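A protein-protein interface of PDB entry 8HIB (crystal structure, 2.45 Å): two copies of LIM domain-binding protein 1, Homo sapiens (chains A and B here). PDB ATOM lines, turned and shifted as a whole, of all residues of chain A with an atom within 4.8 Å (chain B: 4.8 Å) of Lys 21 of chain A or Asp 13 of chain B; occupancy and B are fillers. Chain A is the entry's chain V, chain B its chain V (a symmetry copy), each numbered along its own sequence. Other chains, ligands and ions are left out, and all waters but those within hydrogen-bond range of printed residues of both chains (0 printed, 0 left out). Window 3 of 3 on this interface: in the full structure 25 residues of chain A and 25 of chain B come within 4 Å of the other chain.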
ATOM      1  N   PHE A  17     -24.053   1.682 -22.106  1.00  0.00           N
ATOM      2  CA  PHE A  17     -25.033   1.622 -20.999  1.00  0.00           C
ATOM      3  C   PHE A  17     -26.301   0.948 -21.521  1.00  0.00           C
ATOM      4  O   PHE A  17     -26.881   0.143 -20.815  1.00  0.00           O
ATOM      5  CB  PHE A  17     -25.297   3.023 -20.452  1.00  0.00           C
ATOM      6  CG  PHE A  17     -26.594   3.162 -19.704  1.00  0.00           C
ATOM      7  CD1 PHE A  17     -27.750   3.509 -20.366  1.00  0.00           C
ATOM      8  CD2 PHE A  17     -26.659   2.926 -18.345  1.00  0.00           C
ATOM      9  CE1 PHE A  17     -28.946   3.641 -19.686  1.00  0.00           C
ATOM     10  CE2 PHE A  17     -27.856   3.047 -17.666  1.00  0.00           C
ATOM     11  CZ  PHE A  17     -28.996   3.404 -18.339  1.00  0.00           C
ATOM     12  N   GLU A  18     -26.713   1.289 -22.735  1.00  0.00           N
ATOM     13  CA  GLU A  18     -27.896   0.643 -23.344  1.00  0.00           C
ATOM     14  C   GLU A  18     -27.588  -0.841 -23.540  1.00  0.00           C
ATOM     15  O   GLU A  18     -28.473  -1.654 -23.319  1.00  0.00           O
ATOM     16  CB  GLU A  18     -28.221   1.296 -24.680  1.00  0.00           C
ATOM     17  CG  GLU A  18     -28.800   2.684 -24.550  1.00  0.00           C
ATOM     18  CD  GLU A  18     -29.464   3.179 -25.818  1.00  0.00           C
ATOM     19  OE1 GLU A  18     -28.779   3.269 -26.837  1.00  0.00           O
ATOM     20  OE2 GLU A  18     -30.663   3.454 -25.782  1.00  0.00           O
ATOM     21  N   LEU A  19     -26.368  -1.165 -23.955  1.00  0.00           N
ATOM     22  CA  LEU A  19     -26.004  -2.562 -24.123  1.00  0.00           C
ATOM     23  C   LEU A  19     -26.057  -3.289 -22.780  1.00  0.00           C
ATOM     24  O   LEU A  19     -26.677  -4.351 -22.666  1.00  0.00           O
ATOM     25  CB  LEU A  19     -24.627  -2.681 -24.781  1.00  0.00           C
ATOM     26  CG  LEU A  19     -24.179  -4.117 -25.095  1.00  0.00           C
ATOM     27  CD1 LEU A  19     -23.350  -4.192 -26.372  1.00  0.00           C
ATOM     28  CD2 LEU A  19     -23.391  -4.704 -23.935  1.00  0.00           C
ATOM     29  N   ASN A  20     -25.439  -2.713 -21.738  1.00  0.00           N
ATOM     30  CA  ASN A  20     -25.580  -3.288 -20.399  1.00  0.00           C
ATOM     31  C   ASN A  20     -27.038  -3.437 -20.001  1.00  0.00           C
ATOM     32  O   ASN A  20     -27.418  -4.397 -19.322  1.00  0.00           O
ATOM     33  CB  ASN A  20     -24.898  -2.420 -19.362  1.00  0.00           C
ATOM     34  CG  ASN A  20     -23.422  -2.506 -19.449  1.00  0.00           C
ATOM     35  OD1 ASN A  20     -22.859  -3.480 -19.996  1.00  0.00           O
ATOM     36  ND2 ASN A  20     -22.757  -1.497 -18.915  1.00  0.00           N
ATOM     37  N   LYS A  21     -27.846  -2.457 -20.379  1.00  0.00           N
ATOM     38  CA  LYS A  21     -29.266  -2.478 -19.969  1.00  0.00           C
ATOM     39  C   LYS A  21     -30.013  -3.628 -20.638  1.00  0.00           C
ATOM     40  O   LYS A  21     -30.819  -4.246 -19.960  1.00  0.00           O
ATOM     41  CB  LYS A  21     -29.938  -1.124 -20.194  1.00  0.00           C
ATOM     42  CG  LYS A  21     -31.341  -1.035 -19.626  1.00  0.00           C
ATOM     43  CD  LYS A  21     -31.804   0.364 -19.331  1.00  0.00           C
ATOM     44  CE  LYS A  21     -32.670   0.439 -18.093  1.00  0.00           C
ATOM     45  NZ  LYS A  21     -34.015   0.982 -18.384  1.00  0.00           N
ATOM     46  N   ARG A  22     -29.768  -3.898 -21.915  1.00  0.00           N
ATOM     47  CA  ARG A  22     -30.497  -4.995 -22.524  1.00  0.00           C
ATOM     48  C   ARG A  22     -30.003  -6.337 -22.017  1.00  0.00           C
ATOM     49  O   ARG A  22     -30.793  -7.286 -21.942  1.00  0.00           O
ATOM     50  CB  ARG A  22     -30.457  -4.916 -24.052  1.00  0.00           C
ATOM     51  CG  ARG A  22     -31.813  -4.456 -24.606  1.00  0.00           C
ATOM     52  CD  ARG A  22     -32.186  -5.116 -25.935  1.00  0.00           C
ATOM     53  NE  ARG A  22     -32.794  -6.449 -25.894  1.00  0.00           N
ATOM     54  CZ  ARG A  22     -32.981  -7.193 -26.985  1.00  0.00           C
ATOM     55  NH1 ARG A  22     -32.641  -6.747 -28.190  1.00  0.00           N
ATOM     56  NH2 ARG A  22     -33.513  -8.417 -26.870  1.00  0.00           N
ATOM     57  N   LEU A  23     -28.732  -6.436 -21.623  1.00  0.00           N
ATOM     58  CA  LEU A  23     -28.284  -7.704 -21.057  1.00  0.00           C
ATOM     59  C   LEU A  23     -28.976  -8.012 -19.735  1.00  0.00           C
ATOM     60  O   LEU A  23     -29.086  -9.183 -19.370  1.00  0.00           O
ATOM     61  CB  LEU A  23     -26.753  -7.732 -20.912  1.00  0.00           C
ATOM     62  CG  LEU A  23     -25.984  -7.812 -22.249  1.00  0.00           C
ATOM     63  CD1 LEU A  23     -24.518  -7.446 -22.073  1.00  0.00           C
ATOM     64  CD2 LEU A  23     -26.091  -9.190 -22.847  1.00  0.00           C
ATOM     65  N   GLN A  24     -29.506  -7.011 -19.033  1.00  0.00           N
ATOM     66  CA  GLN A  24     -30.264  -7.309 -17.822  1.00  0.00           C
ATOM     67  C   GLN A  24     -31.596  -8.000 -18.104  1.00  0.00           C
ATOM     68  O   GLN A  24     -32.272  -8.426 -17.158  1.00  0.00           O
ATOM     69  CB  GLN A  24     -30.520  -6.023 -17.034  1.00  0.00           C
ATOM     70  CG  GLN A  24     -29.276  -5.244 -16.774  1.00  0.00           C
ATOM     71  CD  GLN A  24     -29.531  -3.938 -16.069  1.00  0.00           C
ATOM     72  OE1 GLN A  24     -30.559  -3.287 -16.262  1.00  0.00           O
ATOM     73  NE2 GLN A  24     -28.594  -3.547 -15.240  1.00  0.00           N
ATOM     74  N   ASN A  25     -32.009  -8.094 -19.360  1.00  0.00           N
ATOM     75  CA  ASN A  25     -33.231  -8.808 -19.693  1.00  0.00           C
ATOM     76  C   ASN A  25     -33.005 -10.292 -19.874  1.00  0.00           C
ATOM     77  O   ASN A  25     -33.976 -11.023 -20.064  1.00  0.00           O
ATOM     78  CB  ASN A  25     -33.861  -8.219 -20.954  1.00  0.00           C
ATOM     79  CG  ASN A  25     -34.371  -6.842 -20.709  1.00  0.00           C
ATOM     80  OD1 ASN A  25     -34.698  -6.512 -19.578  1.00  0.00           O
ATOM     81  ND2 ASN A  25     -34.345  -5.999 -21.721  1.00  0.00           N
ATOM     82  N   ASN B  10     -34.324   6.895 -20.594  1.00  0.00           N
ATOM     83  CA  ASN B  10     -33.507   7.761 -21.487  1.00  0.00           C
ATOM     84  C   ASN B  10     -33.084   9.025 -20.735  1.00  0.00           C
ATOM     85  O   ASN B  10     -31.991   9.539 -21.015  1.00  0.00           O
ATOM     86  CB  ASN B  10     -34.244   8.139 -22.773  1.00  0.00           C
ATOM     87  CG  ASN B  10     -33.539   9.228 -23.552  1.00  0.00           C
ATOM     88  OD1 ASN B  10     -32.318   9.330 -23.525  1.00  0.00           O
ATOM     89  ND2 ASN B  10     -34.299  10.040 -24.268  1.00  0.00           N
ATOM     90  N   GLN B  11     -33.911   9.524 -19.818  1.00  0.00           N
ATOM     91  CA  GLN B  11     -33.481  10.742 -19.091  1.00  0.00           C
ATOM     92  C   GLN B  11     -32.904  10.342 -17.729  1.00  0.00           C
ATOM     93  O   GLN B  11     -31.699  10.507 -17.540  1.00  0.00           O
ATOM     94  CB  GLN B  11     -34.617  11.762 -18.996  1.00  0.00           C
ATOM     95  CG  GLN B  11     -35.153  12.221 -20.345  1.00  0.00           C
ATOM     96  CD  GLN B  11     -34.482  13.469 -20.862  1.00  0.00           C
ATOM     97  OE1 GLN B  11     -34.083  14.344 -20.100  1.00  0.00           O
ATOM     98  NE2 GLN B  11     -34.356  13.564 -22.175  1.00  0.00           N
ATOM     99  N   THR B  12     -33.731   9.782 -16.847  1.00  0.00           N
ATOM    100  CA  THR B  12     -33.290   9.430 -15.475  1.00  0.00           C
ATOM    101  C   THR B  12     -32.207   8.357 -15.501  1.00  0.00           C
ATOM    102  O   THR B  12     -31.227   8.500 -14.786  1.00  0.00           O
ATOM    103  CB  THR B  12     -34.480   8.954 -14.650  1.00  0.00           C
ATOM    104  OG1 THR B  12     -35.065   7.939 -15.452  1.00  0.00           O
ATOM    105  CG2 THR B  12     -35.484  10.053 -14.422  1.00  0.00           C
ATOM    106  N   ASP B  13     -32.395   7.321 -16.305  1.00  0.00           N
ATOM    107  CA  ASP B  13     -31.414   6.213 -16.399  1.00  0.00           C
ATOM    108  C   ASP B  13     -30.015   6.758 -16.672  1.00  0.00           C
ATOM    109  O   ASP B  13     -29.087   6.346 -16.004  1.00  0.00           O
ATOM    110  CB  ASP B  13     -31.798   5.276 -17.539  1.00  0.00           C
ATOM    111  CG  ASP B  13     -32.247   3.926 -17.046  1.00  0.00           C
ATOM    112  OD1 ASP B  13     -31.850   3.558 -15.942  1.00  0.00           O
ATOM    113  OD2 ASP B  13     -32.972   3.260 -17.778  1.00  0.00           O
ATOM    114  N   TYR B  14     -29.893   7.641 -17.651  1.00  0.00           N
ATOM    115  CA  TYR B  14     -28.587   8.211 -18.048  1.00  0.00           C
ATOM    116  C   TYR B  14     -27.980   9.027 -16.905  1.00  0.00           C
ATOM    117  O   TYR B  14     -26.759   9.031 -16.769  1.00  0.00           O
ATOM    118  CB  TYR B  14     -28.778   9.048 -19.311  1.00  0.00           C
ATOM    119  CG  TYR B  14     -27.511   9.442 -20.019  1.00  0.00           C
ATOM    120  CD1 TYR B  14     -26.607   8.494 -20.457  1.00  0.00           C
ATOM    121  CD2 TYR B  14     -27.219  10.769 -20.251  1.00  0.00           C
ATOM    122  CE1 TYR B  14     -25.448   8.861 -21.114  1.00  0.00           C
ATOM    123  CE2 TYR B  14     -26.060  11.154 -20.895  1.00  0.00           C
ATOM    124  CZ  TYR B  14     -25.172  10.195 -21.327  1.00  0.00           C
ATOM    125  OH  TYR B  14     -24.028  10.570 -21.958  1.00  0.00           O
ATOM    126  N   ARG B  15     -28.809   9.696 -16.106  1.00  0.00           N
ATOM    127  CA  ARG B  15     -28.301  10.523 -14.984  1.00  0.00           C
ATOM    128  C   ARG B  15     -27.499   9.653 -14.016  1.00  0.00           C
ATOM    129  O   ARG B  15     -26.442  10.081 -13.592  1.00  0.00           O
ATOM    130  CB  ARG B  15     -29.454  11.235 -14.284  1.00  0.00           C
ATOM    131  CG  ARG B  15     -30.069  12.343 -15.118  1.00  0.00           C
ATOM    132  CD  ARG B  15     -29.712  13.711 -14.600  1.00  0.00           C
ATOM    133  NE  ARG B  15     -28.361  14.076 -14.954  1.00  0.00           N
ATOM    134  CZ  ARG B  15     -27.643  14.932 -14.264  1.00  0.00           C
ATOM    135  NH1 ARG B  15     -28.160  15.494 -13.194  1.00  0.00           N
ATOM    136  NH2 ARG B  15     -26.418  15.230 -14.642  1.00  0.00           N
ATOM    137  N   ILE B  16     -27.982   8.454 -13.711  1.00  0.00           N
ATOM    138  CA  ILE B  16     -27.233   7.553 -12.796  1.00  0.00           C
ATOM    139  C   ILE B  16     -25.937   7.127 -13.480  1.00  0.00           C
ATOM    140  O   ILE B  16     -24.933   7.010 -12.791  1.00  0.00           O
ATOM    141  CB  ILE B  16     -28.094   6.357 -12.381  1.00  0.00           C
ATOM    142  CG1 ILE B  16     -29.311   6.824 -11.594  1.00  0.00           C
ATOM    143  CG2 ILE B  16     -27.268   5.375 -11.577  1.00  0.00           C
ATOM    144  CD1 ILE B  16     -28.967   7.758 -10.480  1.00  0.00           C
ATOM    145  N   PHE B  17     -25.967   6.914 -14.791  1.00  0.00           N
ATOM    146  CA  PHE B  17     -24.738   6.553 -15.531  1.00  0.00           C
ATOM    147  C   PHE B  17     -23.767   7.728 -15.446  1.00  0.00           C
ATOM    148  O   PHE B  17     -22.583   7.511 -15.262  1.00  0.00           O
ATOM    149  CB  PHE B  17     -25.080   6.179 -16.971  1.00  0.00           C
ATOM    150  CG  PHE B  17     -23.926   6.280 -17.929  1.00  0.00           C
ATOM    151  CD1 PHE B  17     -23.671   7.459 -18.594  1.00  0.00           C
ATOM    152  CD2 PHE B  17     -23.087   5.206 -18.147  1.00  0.00           C
ATOM    153  CE1 PHE B  17     -22.613   7.561 -19.478  1.00  0.00           C
ATOM    154  CE2 PHE B  17     -22.023   5.311 -19.023  1.00  0.00           C
ATOM    155  CZ  PHE B  17     -21.789   6.488 -19.685  1.00  0.00           C
ATOM    156  N   PRO B  91     -35.428  -0.408 -13.491  1.00  0.00           N
ATOM    157  CA  PRO B  91     -36.080   0.652 -12.713  1.00  0.00           C
ATOM    158  C   PRO B  91     -37.347   1.165 -13.387  1.00  0.00           C
ATOM    159  O   PRO B  91     -37.433   1.234 -14.612  1.00  0.00           O
ATOM    160  CB  PRO B  91     -35.009   1.747 -12.636  1.00  0.00           C
ATOM    161  CG  PRO B  91     -34.233   1.567 -13.889  1.00  0.00           C
ATOM    162  CD  PRO B  91     -34.185   0.077 -14.127  1.00  0.00           C
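Phe 17 of chain B touches its own counterpart, Phe 17 of chain A. Position printed for both chains: 17. Of the 3 pairs that touch across the chains among the printed residues, 1 has its exchanged pair printed and touching as well.
The side-chain amino group (NZ) of Lys 21 of chain A is in salt-bridge range of the side-chain carboxylate (OD2) of Asp 13 of chain B.
Among the printed residues, merely in contact across the chains: Phe 17 of chain A with Asp 13 of chain B and Phe 17 of chain A with Phe 17 of chain B.
Of chain B, only Asp 13 comes within 4 Å of Lys 21 of chain A. Of the printed residues of chain A, Asp 13 of chain B touches Phe 17 (3.5 Å) and Lys 21 (2.6 Å). Printed residues of chain B within 4 Å of Phe 17 of chain A: Asp 13 and Phe 17. Of the printed residues of chain A, Phe 17 of chain B touches Phe 17.
Hydrophobic or aromatic side chains of chain B that line the printed part of chain A: Phe 17. Among the printed residues, Asp or Glu carboxylates within 4 Å of a Lys or Arg side-chain nitrogen of the other chain: Lys 21 of chain A with Asp 13 of chain B (2.6 Å).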
